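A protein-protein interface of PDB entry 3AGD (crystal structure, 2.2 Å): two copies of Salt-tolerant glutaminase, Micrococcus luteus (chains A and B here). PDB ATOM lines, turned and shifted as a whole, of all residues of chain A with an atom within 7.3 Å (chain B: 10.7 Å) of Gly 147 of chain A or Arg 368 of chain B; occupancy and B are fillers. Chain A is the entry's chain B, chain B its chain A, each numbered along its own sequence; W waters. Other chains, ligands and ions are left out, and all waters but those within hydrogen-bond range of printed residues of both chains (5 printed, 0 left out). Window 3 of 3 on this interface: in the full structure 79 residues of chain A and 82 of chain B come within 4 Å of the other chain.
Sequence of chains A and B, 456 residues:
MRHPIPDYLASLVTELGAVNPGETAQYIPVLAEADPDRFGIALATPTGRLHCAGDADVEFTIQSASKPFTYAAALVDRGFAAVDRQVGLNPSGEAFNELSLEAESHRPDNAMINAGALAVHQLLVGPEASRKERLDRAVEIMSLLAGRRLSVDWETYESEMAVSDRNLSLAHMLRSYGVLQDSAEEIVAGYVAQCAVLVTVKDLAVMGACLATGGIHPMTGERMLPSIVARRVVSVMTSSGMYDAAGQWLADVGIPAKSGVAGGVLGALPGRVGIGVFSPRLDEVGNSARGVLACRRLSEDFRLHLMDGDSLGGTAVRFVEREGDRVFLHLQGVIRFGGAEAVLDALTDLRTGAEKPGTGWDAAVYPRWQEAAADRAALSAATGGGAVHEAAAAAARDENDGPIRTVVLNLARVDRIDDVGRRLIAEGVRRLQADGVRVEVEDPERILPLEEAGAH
The backbone carbonyl oxygen (O) of Ser 143 of chain A sits at hydrogen-bond distance from the backbone NH (N) of Arg 148 of chain A (3.1 Å).
The guanidinium group of Arg 148 of chain A lies within salt-bridge range of the side-chain carboxylate of Asp 203 of chain A, 2.7 Å away.
O of Glu 222 of chain A lies within hydrogen-bond range of N of His 217 of chain A (2.9 Å).
A ring nitrogen (ND1) of His 217 of chain A sits at hydrogen-bond distance from the backbone NH (N) of Met 219 of chain A.
The backbone carbonyl oxygen of Leu 145 of chain A sits at hydrogen-bond distance from a ring nitrogen (NE2) of His 217 of chain A (3.3 Å).
OG1 of Thr 220 of chain A sits close to N of Glu 222 of chain A (3.1 Å).
Among the printed residues, merely in contact across the chains: Gly 147 of chain A with Tyr 366 of chain B (3.4 Å), Met 219 of chain A with Trp 369 of chain B (3.4 Å), Arg 148 of chain A with Tyr 366 of chain B (3.4 Å), Met 219 of chain A with Ala 372 of chain B (3.4 Å), His 217 of chain A with Trp 369 of chain B (3.5 Å), Thr 220 of chain A with Leu 379 of chain B (3.5 Å), Thr 220 of chain A with Trp 369 of chain B (3.5 Å), Ala 146 of chain A with Trp 369 of chain B (3.5 Å), Gly 147 of chain A with Arg 368 of chain B (3.5 Å) and Thr 220 of chain A with Ala 372 of chain B (3.7 Å).
Of the printed residues of chain B, Gly 147 of chain A touches Tyr 366 (3.4 Å) and Arg 368 (3.5 Å).
Of chain A, only Gly 147 comes within 4 Å of Arg 368 of chain B.
Thr 220 of chain A touches just these residues of chain B: Trp 369, Ala 372 and Leu 379.
Of the printed residues of chain B, His 217 of chain A touches Trp 369 (3.5 Å).
Printed residues of chain A within 4 Å of Leu 379 of chain B: Thr 220.
Of the printed residues of chain A, Tyr 366 of chain B touches Gly 147 (3.4 Å) and Arg 148 (3.4 Å).
Ala 364 of chain B touches none of the printed residues of chain A.
Asp 203 of chain A touches none of the printed residues of chain B.
Printed residues of chain B that touch a printed residue of chain A: Tyr 366, Arg 368, Trp 369, Ala 372 and Leu 379.
Hydrophobic or aromatic side chains of chain B within 4 Å of the printed part of chain A: Tyr 366, Trp 369, Ala 372 and Leu 379.
Among the printed residues, no Asp or Glu carboxylate lies within 4 Å of a Lys or Arg side-chain nitrogen of the other chain.
No position is printed for both chains.
Water W1 lies within hydrogen-bond range of NH1 of Arg 368 of chain B (2.5 Å), O of Gly 147 of chain A (2.7 Å) and NE1 of Trp 369 of chain B (3.1 Å).
Water W5 bridges the backbone carbonyl oxygen (O) of Val 365 of chain B and the backbone carbonyl oxygen (O) of Gly 147 of chain A.
Water W4 lies within hydrogen-bond range of the backbone carbonyl oxygen (O) of Ala 146 of chain A (2.7 Å), the side-chain carboxylate (OD1) of Asp 203 of chain A (2.9 Å) and the side-chain hydroxyl (OH) of Tyr 366 of chain B (3.0 Å).
Water W3 lies within hydrogen-bond range of the backbone carbonyl oxygen of Thr 220 of chain A (3.1 Å) and the backbone NH of Leu 379 of chain B (3.2 Å).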
ATOM      1  N   ILE A 141      35.376  26.815 -11.584  1.00  0.00           N
ATOM      2  CA  ILE A 141      34.793  26.223 -10.385  1.00  0.00           C
ATOM      3  C   ILE A 141      33.437  26.849 -10.048  1.00  0.00           C
ATOM      4  O   ILE A 141      32.466  26.139  -9.764  1.00  0.00           O
ATOM      5  CB  ILE A 141      35.744  26.329  -9.159  1.00  0.00           C
ATOM      6  CG1 ILE A 141      35.175  25.493  -8.013  1.00  0.00           C
ATOM      7  CG2 ILE A 141      35.916  27.777  -8.721  1.00  0.00           C
ATOM      8  CD1 ILE A 141      34.943  24.034  -8.388  1.00  0.00           C
ATOM      9  N   MET A 142      33.369  28.175 -10.096  1.00  0.00           N
ATOM     10  CA  MET A 142      32.128  28.876  -9.810  1.00  0.00           C
ATOM     11  C   MET A 142      31.056  28.550 -10.853  1.00  0.00           C
ATOM     12  O   MET A 142      29.885  28.364 -10.507  1.00  0.00           O
ATOM     13  CB  MET A 142      32.391  30.384  -9.732  1.00  0.00           C
ATOM     14  CG  MET A 142      33.068  30.793  -8.423  1.00  0.00           C
ATOM     15  SD  MET A 142      33.588  32.515  -8.324  1.00  0.00           S
ATOM     16  CE  MET A 142      32.067  33.326  -8.362  1.00  0.00           C
ATOM     17  N   SER A 143      31.454  28.460 -12.120  1.00  0.00           N
ATOM     18  CA  SER A 143      30.505  28.138 -13.189  1.00  0.00           C
ATOM     19  C   SER A 143      29.981  26.704 -13.061  1.00  0.00           C
ATOM     20  O   SER A 143      28.798  26.445 -13.283  1.00  0.00           O
ATOM     21  CB  SER A 143      31.156  28.306 -14.566  1.00  0.00           C
ATOM     22  OG  SER A 143      31.497  29.658 -14.826  1.00  0.00           O
ATOM     23  N   LEU A 144      30.867  25.775 -12.711  1.00  0.00           N
ATOM     24  CA  LEU A 144      30.483  24.372 -12.561  1.00  0.00           C
ATOM     25  C   LEU A 144      29.477  24.168 -11.434  1.00  0.00           C
ATOM     26  O   LEU A 144      28.515  23.410 -11.583  1.00  0.00           O
ATOM     27  CB  LEU A 144      31.716  23.503 -12.303  1.00  0.00           C
ATOM     28  CG  LEU A 144      32.668  23.275 -13.478  1.00  0.00           C
ATOM     29  CD1 LEU A 144      33.881  22.474 -13.016  1.00  0.00           C
ATOM     30  CD2 LEU A 144      31.933  22.536 -14.588  1.00  0.00           C
ATOM     31  N   LEU A 145      29.698  24.834 -10.305  1.00  0.00           N
ATOM     32  CA  LEU A 145      28.788  24.706  -9.171  1.00  0.00           C
ATOM     33  C   LEU A 145      27.492  25.476  -9.425  1.00  0.00           C
ATOM     34  O   LEU A 145      26.435  25.097  -8.926  1.00  0.00           O
ATOM     35  CB  LEU A 145      29.456  25.202  -7.882  1.00  0.00           C
ATOM     36  CG  LEU A 145      30.793  24.550  -7.502  1.00  0.00           C
ATOM     37  CD1 LEU A 145      31.138  24.916  -6.070  1.00  0.00           C
ATOM     38  CD2 LEU A 145      30.712  23.038  -7.640  1.00  0.00           C
ATOM     39  N   ALA A 146      27.575  26.552 -10.204  1.00  0.00           N
ATOM     40  CA  ALA A 146      26.393  27.349 -10.521  1.00  0.00           C
ATOM     41  C   ALA A 146      25.553  26.651 -11.589  1.00  0.00           C
ATOM     42  O   ALA A 146      24.348  26.883 -11.691  1.00  0.00           O
ATOM     43  CB  ALA A 146      26.800  28.735 -11.010  1.00  0.00           C
ATOM     44  N   GLY A 147      26.199  25.805 -12.386  1.00  0.00           N
ATOM     45  CA  GLY A 147      25.490  25.088 -13.428  1.00  0.00           C
ATOM     46  C   GLY A 147      25.413  25.821 -14.757  1.00  0.00           C
ATOM     47  O   GLY A 147      24.677  25.407 -15.653  1.00  0.00           O
ATOM     48  N   ARG A 148      26.162  26.912 -14.889  1.00  0.00           N
ATOM     49  CA  ARG A 148      26.174  27.688 -16.126  1.00  0.00           C
ATOM     50  C   ARG A 148      27.458  28.499 -16.206  1.00  0.00           C
ATOM     51  O   ARG A 148      28.087  28.772 -15.186  1.00  0.00           O
ATOM     52  CB  ARG A 148      24.964  28.622 -16.191  1.00  0.00           C
ATOM     53  CG  ARG A 148      24.995  29.786 -15.212  1.00  0.00           C
ATOM     54  CD  ARG A 148      23.710  30.611 -15.292  1.00  0.00           C
ATOM     55  NE  ARG A 148      23.774  31.809 -14.457  1.00  0.00           N
ATOM     56  CZ  ARG A 148      24.268  32.978 -14.854  1.00  0.00           C
ATOM     57  NH1 ARG A 148      24.292  34.010 -14.018  1.00  0.00           N
ATOM     58  NH2 ARG A 148      24.723  33.124 -16.092  1.00  0.00           N
ATOM     59  N   ARG A 149      27.852  28.880 -17.418  1.00  0.00           N
ATOM     60  CA  ARG A 149      29.071  29.654 -17.595  1.00  0.00           C
ATOM     61  C   ARG A 149      28.887  31.092 -17.119  1.00  0.00           C
ATOM     62  O   ARG A 149      28.027  31.820 -17.613  1.00  0.00           O
ATOM     63  CB  ARG A 149      29.518  29.620 -19.060  1.00  0.00           C
ATOM     64  CG  ARG A 149      30.730  30.498 -19.352  1.00  0.00           C
ATOM     65  CD  ARG A 149      31.713  30.520 -18.178  1.00  0.00           C
ATOM     66  NE  ARG A 149      33.009  29.950 -18.522  1.00  0.00           N
ATOM     67  CZ  ARG A 149      33.609  28.981 -17.836  1.00  0.00           C
ATOM     68  NH1 ARG A 149      33.038  28.466 -16.760  1.00  0.00           N
ATOM     69  NH2 ARG A 149      34.783  28.521 -18.232  1.00  0.00           N
ATOM     70  N   LEU A 150      29.702  31.489 -16.147  1.00  0.00           N
ATOM     71  CA  LEU A 150      29.634  32.829 -15.580  1.00  0.00           C
ATOM     72  C   LEU A 150      30.636  33.748 -16.253  1.00  0.00           C
ATOM     73  O   LEU A 150      31.608  33.288 -16.844  1.00  0.00           O
ATOM     74  CB  LEU A 150      29.915  32.768 -14.077  1.00  0.00           C
ATOM     75  CG  LEU A 150      29.024  31.790 -13.306  1.00  0.00           C
ATOM     76  CD1 LEU A 150      29.485  31.681 -11.857  1.00  0.00           C
ATOM     77  CD2 LEU A 150      27.584  32.265 -13.383  1.00  0.00           C
ATOM     78  N   ASP A 203      22.095  31.977  -8.413  1.00  0.00           N
ATOM     79  CA  ASP A 203      23.388  31.328  -8.643  1.00  0.00           C
ATOM     80  C   ASP A 203      24.011  30.959  -7.302  1.00  0.00           C
ATOM     81  O   ASP A 203      24.411  29.821  -7.091  1.00  0.00           O
ATOM     82  CB  ASP A 203      24.365  32.251  -9.390  1.00  0.00           C
ATOM     83  CG  ASP A 203      24.014  32.433 -10.861  1.00  0.00           C
ATOM     84  OD1 ASP A 203      23.716  31.427 -11.538  1.00  0.00           O
ATOM     85  OD2 ASP A 203      24.058  33.587 -11.343  1.00  0.00           O
ATOM     86  N   VAL A 206      22.383  27.924  -5.515  1.00  0.00           N
ATOM     87  CA  VAL A 206      22.771  26.640  -6.085  1.00  0.00           C
ATOM     88  C   VAL A 206      24.211  26.305  -5.740  1.00  0.00           C
ATOM     89  O   VAL A 206      24.528  25.162  -5.402  1.00  0.00           O
ATOM     90  CB  VAL A 206      22.619  26.621  -7.615  1.00  0.00           C
ATOM     91  CG1 VAL A 206      23.061  25.263  -8.161  1.00  0.00           C
ATOM     92  CG2 VAL A 206      21.164  26.884  -7.993  1.00  0.00           C
ATOM     93  N   MET A 207      25.084  27.303  -5.830  1.00  0.00           N
ATOM     94  CA  MET A 207      26.493  27.103  -5.513  1.00  0.00           C
ATOM     95  C   MET A 207      26.605  26.712  -4.041  1.00  0.00           C
ATOM     96  O   MET A 207      27.367  25.815  -3.685  1.00  0.00           O
ATOM     97  CB  MET A 207      27.272  28.386  -5.796  1.00  0.00           C
ATOM     98  CG  MET A 207      27.242  28.788  -7.262  1.00  0.00           C
ATOM     99  SD  MET A 207      27.777  30.487  -7.548  1.00  0.00           S
ATOM    100  CE  MET A 207      29.562  30.339  -7.361  1.00  0.00           C
ATOM    101  N   CYS A 210      25.550  23.117  -3.441  1.00  0.00           N
ATOM    102  CA  CYS A 210      26.585  22.145  -3.804  1.00  0.00           C
ATOM    103  C   CYS A 210      27.499  21.842  -2.613  1.00  0.00           C
ATOM    104  O   CYS A 210      28.007  20.731  -2.480  1.00  0.00           O
ATOM    105  CB  CYS A 210      27.437  22.665  -4.963  1.00  0.00           C
ATOM    106  SG  CYS A 210      26.651  22.570  -6.574  1.00  0.00           S
ATOM    107  N   HIS A 217      25.793  18.223  -6.790  1.00  0.00           N
ATOM    108  CA  HIS A 217      24.969  19.245  -7.417  1.00  0.00           C
ATOM    109  C   HIS A 217      23.507  18.822  -7.284  1.00  0.00           C
ATOM    110  O   HIS A 217      23.114  17.769  -7.774  1.00  0.00           O
ATOM    111  CB  HIS A 217      25.331  19.410  -8.890  1.00  0.00           C
ATOM    112  CG  HIS A 217      24.840  20.694  -9.475  1.00  0.00           C
ATOM    113  ND1 HIS A 217      23.499  20.996  -9.583  1.00  0.00           N
ATOM    114  CD2 HIS A 217      25.509  21.789  -9.906  1.00  0.00           C
ATOM    115  CE1 HIS A 217      23.363  22.223 -10.053  1.00  0.00           C
ATOM    116  NE2 HIS A 217      24.567  22.728 -10.257  1.00  0.00           N
ATOM    117  N   MET A 219      20.846  19.817  -8.759  1.00  0.00           N
ATOM    118  CA  MET A 219      20.041  19.789  -9.975  1.00  0.00           C
ATOM    119  C   MET A 219      20.378  18.634 -10.904  1.00  0.00           C
ATOM    120  O   MET A 219      19.604  18.316 -11.803  1.00  0.00           O
ATOM    121  CB  MET A 219      20.195  21.100 -10.744  1.00  0.00           C
ATOM    122  CG  MET A 219      19.827  22.346  -9.961  1.00  0.00           C
ATOM    123  SD  MET A 219      18.132  22.342  -9.371  1.00  0.00           S
ATOM    124  CE  MET A 219      18.405  22.401  -7.618  1.00  0.00           C
ATOM    125  N   THR A 220      21.527  18.003 -10.696  1.00  0.00           N
ATOM    126  CA  THR A 220      21.928  16.899 -11.562  1.00  0.00           C
ATOM    127  C   THR A 220      22.300  15.639 -10.803  1.00  0.00           C
ATOM    128  O   THR A 220      22.304  14.548 -11.372  1.00  0.00           O
ATOM    129  CB  THR A 220      23.134  17.286 -12.434  1.00  0.00           C
ATOM    130  OG1 THR A 220      24.273  17.506 -11.594  1.00  0.00           O
ATOM    131  CG2 THR A 220      22.837  18.553 -13.222  1.00  0.00           C
ATOM    132  N   GLU A 222      25.142  15.081  -9.806  1.00  0.00           N
ATOM    133  CA  GLU A 222      26.545  14.811 -10.110  1.00  0.00           C
ATOM    134  C   GLU A 222      27.440  15.315  -8.978  1.00  0.00           C
ATOM    135  O   GLU A 222      27.233  16.409  -8.460  1.00  0.00           O
ATOM    136  CB  GLU A 222      26.953  15.496 -11.418  1.00  0.00           C
ATOM    137  CG  GLU A 222      28.415  15.282 -11.804  1.00  0.00           C
ATOM    138  CD  GLU A 222      28.916  16.291 -12.839  1.00  0.00           C
ATOM    139  OE1 GLU A 222      28.348  16.351 -13.947  1.00  0.00           O
ATOM    140  OE2 GLU A 222      29.879  17.030 -12.549  1.00  0.00           O
ATOM    141  N   MET A 224      30.277  17.168  -7.613  1.00  0.00           N
ATOM    142  CA  MET A 224      31.133  18.242  -8.087  1.00  0.00           C
ATOM    143  C   MET A 224      32.406  18.379  -7.267  1.00  0.00           C
ATOM    144  O   MET A 224      33.435  18.820  -7.784  1.00  0.00           O
ATOM    145  CB  MET A 224      30.359  19.558  -8.046  1.00  0.00           C
ATOM    146  CG  MET A 224      28.988  19.467  -8.693  1.00  0.00           C
ATOM    147  SD  MET A 224      29.134  18.878 -10.380  1.00  0.00           S
ATOM    148  CE  MET A 224      29.777  20.341 -11.172  1.00  0.00           C
ATOM    149  N   TRP B 361      14.083  27.951 -13.150  1.00  0.00           N
ATOM    150  CA  TRP B 361      15.186  28.054 -14.098  1.00  0.00           C
ATOM    151  C   TRP B 361      14.712  27.851 -15.539  1.00  0.00           C
ATOM    152  O   TRP B 361      13.610  27.359 -15.776  1.00  0.00           O
ATOM    153  CB  TRP B 361      16.278  27.027 -13.763  1.00  0.00           C
ATOM    154  CG  TRP B 361      15.804  25.597 -13.732  1.00  0.00           C
ATOM    155  CD1 TRP B 361      15.124  24.976 -12.722  1.00  0.00           C
ATOM    156  CD2 TRP B 361      15.970  24.615 -14.765  1.00  0.00           C
ATOM    157  NE1 TRP B 361      14.858  23.669 -13.061  1.00  0.00           N
ATOM    158  CE2 TRP B 361      15.365  23.421 -14.309  1.00  0.00           C
ATOM    159  CE3 TRP B 361      16.570  24.628 -16.031  1.00  0.00           C
ATOM    160  CZ2 TRP B 361      15.345  22.250 -15.076  1.00  0.00           C
ATOM    161  CZ3 TRP B 361      16.549  23.461 -16.794  1.00  0.00           C
ATOM    162  CH2 TRP B 361      15.940  22.290 -16.311  1.00  0.00           C
ATOM    163  N   ASP B 362      15.554  28.233 -16.495  1.00  0.00           N
ATOM    164  CA  ASP B 362      15.227  28.098 -17.911  1.00  0.00           C
ATOM    165  C   ASP B 362      15.783  26.789 -18.473  1.00  0.00           C
ATOM    166  O   ASP B 362      16.994  26.575 -18.488  1.00  0.00           O
ATOM    167  CB  ASP B 362      15.802  29.284 -18.689  1.00  0.00           C
ATOM    168  CG  ASP B 362      15.300  29.348 -20.120  1.00  0.00           C
ATOM    169  OD1 ASP B 362      15.474  28.361 -20.864  1.00  0.00           O
ATOM    170  OD2 ASP B 362      14.730  30.393 -20.500  1.00  0.00           O
ATOM    171  N   ALA B 363      14.889  25.919 -18.938  1.00  0.00           N
ATOM    172  CA  ALA B 363      15.278  24.625 -19.491  1.00  0.00           C
ATOM    173  C   ALA B 363      16.268  24.746 -20.646  1.00  0.00           C
ATOM    174  O   ALA B 363      17.124  23.880 -20.832  1.00  0.00           O
ATOM    175  CB  ALA B 363      14.041  23.859 -19.944  1.00  0.00           C
ATOM    176  N   ALA B 364      16.142  25.817 -21.425  1.00  0.00           N
ATOM    177  CA  ALA B 364      17.034  26.043 -22.557  1.00  0.00           C
ATOM    178  C   ALA B 364      18.394  26.516 -22.056  1.00  0.00           C
ATOM    179  O   ALA B 364      19.394  26.431 -22.769  1.00  0.00           O
ATOM    180  CB  ALA B 364      16.432  27.079 -23.504  1.00  0.00           C
ATOM    181  N   VAL B 365      18.421  27.015 -20.823  1.00  0.00           N
ATOM    182  CA  VAL B 365      19.654  27.505 -20.216  1.00  0.00           C
ATOM    183  C   VAL B 365      20.413  26.377 -19.527  1.00  0.00           C
ATOM    184  O   VAL B 365      21.642  26.339 -19.558  1.00  0.00           O
ATOM    185  CB  VAL B 365      19.363  28.621 -19.183  1.00  0.00           C
ATOM    186  CG1 VAL B 365      20.647  29.035 -18.479  1.00  0.00           C
ATOM    187  CG2 VAL B 365      18.745  29.821 -19.879  1.00  0.00           C
ATOM    188  N   TYR B 366      19.681  25.455 -18.908  1.00  0.00           N
ATOM    189  CA  TYR B 366      20.308  24.334 -18.216  1.00  0.00           C
ATOM    190  C   TYR B 366      19.855  22.989 -18.783  1.00  0.00           C
ATOM    191  O   TYR B 366      19.145  22.233 -18.117  1.00  0.00           O
ATOM    192  CB  TYR B 366      19.980  24.371 -16.721  1.00  0.00           C
ATOM    193  CG  TYR B 366      20.220  25.698 -16.039  1.00  0.00           C
ATOM    194  CD1 TYR B 366      19.265  26.715 -16.090  1.00  0.00           C
ATOM    195  CD2 TYR B 366      21.384  25.926 -15.307  1.00  0.00           C
ATOM    196  CE1 TYR B 366      19.460  27.925 -15.421  1.00  0.00           C
ATOM    197  CE2 TYR B 366      21.592  27.131 -14.636  1.00  0.00           C
ATOM    198  CZ  TYR B 366      20.625  28.123 -14.695  1.00  0.00           C
ATOM    199  OH  TYR B 366      20.817  29.301 -14.010  1.00  0.00           O
ATOM    200  N   PRO B 367      20.263  22.668 -20.022  1.00  0.00           N
ATOM    201  CA  PRO B 367      19.863  21.390 -20.620  1.00  0.00           C
ATOM    202  C   PRO B 367      20.237  20.168 -19.772  1.00  0.00           C
ATOM    203  O   PRO B 367      19.541  19.151 -19.803  1.00  0.00           O
ATOM    204  CB  PRO B 367      20.569  21.408 -21.982  1.00  0.00           C
ATOM    205  CG  PRO B 367      21.764  22.297 -21.746  1.00  0.00           C
ATOM    206  CD  PRO B 367      21.168  23.408 -20.918  1.00  0.00           C
ATOM    207  N   ARG B 368      21.328  20.270 -19.017  1.00  0.00           N
ATOM    208  CA  ARG B 368      21.768  19.166 -18.166  1.00  0.00           C
ATOM    209  C   ARG B 368      20.792  18.969 -17.010  1.00  0.00           C
ATOM    210  O   ARG B 368      20.553  17.842 -16.574  1.00  0.00           O
ATOM    211  CB  ARG B 368      23.169  19.432 -17.607  1.00  0.00           C
ATOM    212  CG  ARG B 368      24.205  19.797 -18.654  1.00  0.00           C
ATOM    213  CD  ARG B 368      25.614  19.765 -18.078  1.00  0.00           C
ATOM    214  NE  ARG B 368      26.473  20.767 -18.700  1.00  0.00           N
ATOM    215  CZ  ARG B 368      26.461  22.060 -18.385  1.00  0.00           C
ATOM    216  NH1 ARG B 368      25.638  22.511 -17.448  1.00  0.00           N
ATOM    217  NH2 ARG B 368      27.263  22.906 -19.016  1.00  0.00           N
ATOM    218  N   TRP B 369      20.235  20.073 -16.517  1.00  0.00           N
ATOM    219  CA  TRP B 369      19.274  20.026 -15.418  1.00  0.00           C
ATOM    220  C   TRP B 369      17.989  19.349 -15.887  1.00  0.00           C
ATOM    221  O   TRP B 369      17.336  18.637 -15.121  1.00  0.00           O
ATOM    222  CB  TRP B 369      18.971  21.444 -14.916  1.00  0.00           C
ATOM    223  CG  TRP B 369      20.105  22.084 -14.152  1.00  0.00           C
ATOM    224  CD1 TRP B 369      21.401  21.648 -14.080  1.00  0.00           C
ATOM    225  CD2 TRP B 369      20.045  23.288 -13.373  1.00  0.00           C
ATOM    226  NE1 TRP B 369      22.149  22.506 -13.307  1.00  0.00           N
ATOM    227  CE2 TRP B 369      21.344  23.520 -12.861  1.00  0.00           C
ATOM    228  CE3 TRP B 369      19.021  24.193 -13.060  1.00  0.00           C
ATOM    229  CZ2 TRP B 369      21.646  24.625 -12.051  1.00  0.00           C
ATOM    230  CZ3 TRP B 369      19.322  25.293 -12.251  1.00  0.00           C
ATOM    231  CH2 TRP B 369      20.625  25.497 -11.759  1.00  0.00           C
ATOM    232  N   GLN B 370      17.634  19.576 -17.149  1.00  0.00           N
ATOM    233  CA  GLN B 370      16.436  18.980 -17.731  1.00  0.00           C
ATOM    234  C   GLN B 370      16.625  17.473 -17.871  1.00  0.00           C
ATOM    235  O   GLN B 370      15.790  16.691 -17.420  1.00  0.00           O
ATOM    236  CB  GLN B 370      16.155  19.583 -19.107  1.00  0.00           C
ATOM    237  CG  GLN B 370      14.973  18.949 -19.823  1.00  0.00           C
ATOM    238  CD  GLN B 370      14.871  19.377 -21.273  1.00  0.00           C
ATOM    239  OE1 GLN B 370      14.739  20.563 -21.576  1.00  0.00           O
ATOM    240  NE2 GLN B 370      14.933  18.409 -22.181  1.00  0.00           N
ATOM    241  N   GLU B 371      17.727  17.076 -18.505  1.00  0.00           N
ATOM    242  CA  GLU B 371      18.034  15.663 -18.700  1.00  0.00           C
ATOM    243  C   GLU B 371      17.976  14.915 -17.375  1.00  0.00           C
ATOM    244  O   GLU B 371      17.431  13.814 -17.297  1.00  0.00           O
ATOM    245  CB  GLU B 371      19.429  15.496 -19.305  1.00  0.00           C
ATOM    246  CG  GLU B 371      19.575  16.018 -20.720  1.00  0.00           C
ATOM    247  CD  GLU B 371      20.971  15.801 -21.267  1.00  0.00           C
ATOM    248  OE1 GLU B 371      21.419  14.633 -21.297  1.00  0.00           O
ATOM    249  OE2 GLU B 371      21.620  16.794 -21.663  1.00  0.00           O
ATOM    250  N   ALA B 372      18.549  15.517 -16.336  1.00  0.00           N
ATOM    251  CA  ALA B 372      18.561  14.912 -15.011  1.00  0.00           C
ATOM    252  C   ALA B 372      17.140  14.822 -14.459  1.00  0.00           C
ATOM    253  O   ALA B 372      16.748  13.801 -13.887  1.00  0.00           O
ATOM    254  CB  ALA B 372      19.442  15.731 -14.071  1.00  0.00           C
ATOM    255  N   ALA B 373      16.373  15.895 -14.640  1.00  0.00           N
ATOM    256  CA  ALA B 373      14.995  15.947 -14.166  1.00  0.00           C
ATOM    257  C   ALA B 373      14.127  14.954 -14.933  1.00  0.00           C
ATOM    258  O   ALA B 373      12.967  14.733 -14.584  1.00  0.00           O
ATOM    259  CB  ALA B 373      14.441  17.358 -14.322  1.00  0.00           C
ATOM    260  N   ALA B 374      14.694  14.362 -15.982  1.00  0.00           N
ATOM    261  CA  ALA B 374      13.975  13.382 -16.791  1.00  0.00           C
ATOM    262  C   ALA B 374      13.974  12.038 -16.067  1.00  0.00           C
ATOM    263  O   ALA B 374      12.921  11.423 -15.884  1.00  0.00           O
ATOM    264  CB  ALA B 374      14.634  13.243 -18.163  1.00  0.00           C
ATOM    265  N   ASP B 375      15.158  11.585 -15.663  1.00  0.00           N
ATOM    266  CA  ASP B 375      15.280  10.325 -14.940  1.00  0.00           C
ATOM    267  C   ASP B 375      15.079  10.658 -13.466  1.00  0.00           C
ATOM    268  O   ASP B 375      16.004  10.577 -12.654  1.00  0.00           O
ATOM    269  CB  ASP B 375      16.660   9.701 -15.150  1.00  0.00           C
ATOM    270  CG  ASP B 375      16.689   8.225 -14.793  1.00  0.00           C
ATOM    271  OD1 ASP B 375      16.141   7.858 -13.732  1.00  0.00           O
ATOM    272  OD2 ASP B 375      17.261   7.433 -15.570  1.00  0.00           O
ATOM    273  N   ARG B 376      13.851  11.048 -13.146  1.00  0.00           N
ATOM    274  CA  ARG B 376      13.450  11.431 -11.803  1.00  0.00           C
ATOM    275  C   ARG B 376      13.965  10.507 -10.696  1.00  0.00           C
ATOM    276  O   ARG B 376      14.541  10.975  -9.713  1.00  0.00           O
ATOM    277  CB  ARG B 376      11.923  11.520 -11.758  1.00  0.00           C
ATOM    278  CG  ARG B 376      11.350  12.024 -10.458  1.00  0.00           C
ATOM    279  CD  ARG B 376       9.853  12.299 -10.569  1.00  0.00           C
ATOM    280  NE  ARG B 376       9.105  11.185 -11.150  1.00  0.00           N
ATOM    281  CZ  ARG B 376       8.893  11.022 -12.453  1.00  0.00           C
ATOM    282  NH1 ARG B 376       9.371  11.902 -13.321  1.00  0.00           N
ATOM    283  NH2 ARG B 376       8.199   9.978 -12.890  1.00  0.00           N
ATOM    284  N   LEU B 379      17.902  10.809 -10.276  1.00  0.00           N
ATOM    285  CA  LEU B 379      18.253  12.085  -9.667  1.00  0.00           C
ATOM    286  C   LEU B 379      17.974  12.053  -8.166  1.00  0.00           C
ATOM    287  O   LEU B 379      18.728  12.618  -7.374  1.00  0.00           O
ATOM    288  CB  LEU B 379      17.456  13.216 -10.330  1.00  0.00           C
ATOM    289  CG  LEU B 379      17.597  14.660  -9.824  1.00  0.00           C
ATOM    290  CD1 LEU B 379      16.800  14.847  -8.541  1.00  0.00           C
ATOM    291  CD2 LEU B 379      19.068  14.998  -9.615  1.00  0.00           C
HETATM  292  O   HOH W   1      23.578  22.993 -16.026  1.00  0.00           O
HETATM  293  O   HOH W   2      17.214  19.204 -12.511  1.00  0.00           O
HETATM  294  O   HOH W   3      20.774  11.877 -11.282  1.00  0.00           O
HETATM  295  O   HOH W   4      22.536  28.814 -11.570  1.00  0.00           O
HETATM  296  O   HOH W   5      23.918  25.897 -18.417  1.00  0.00           O
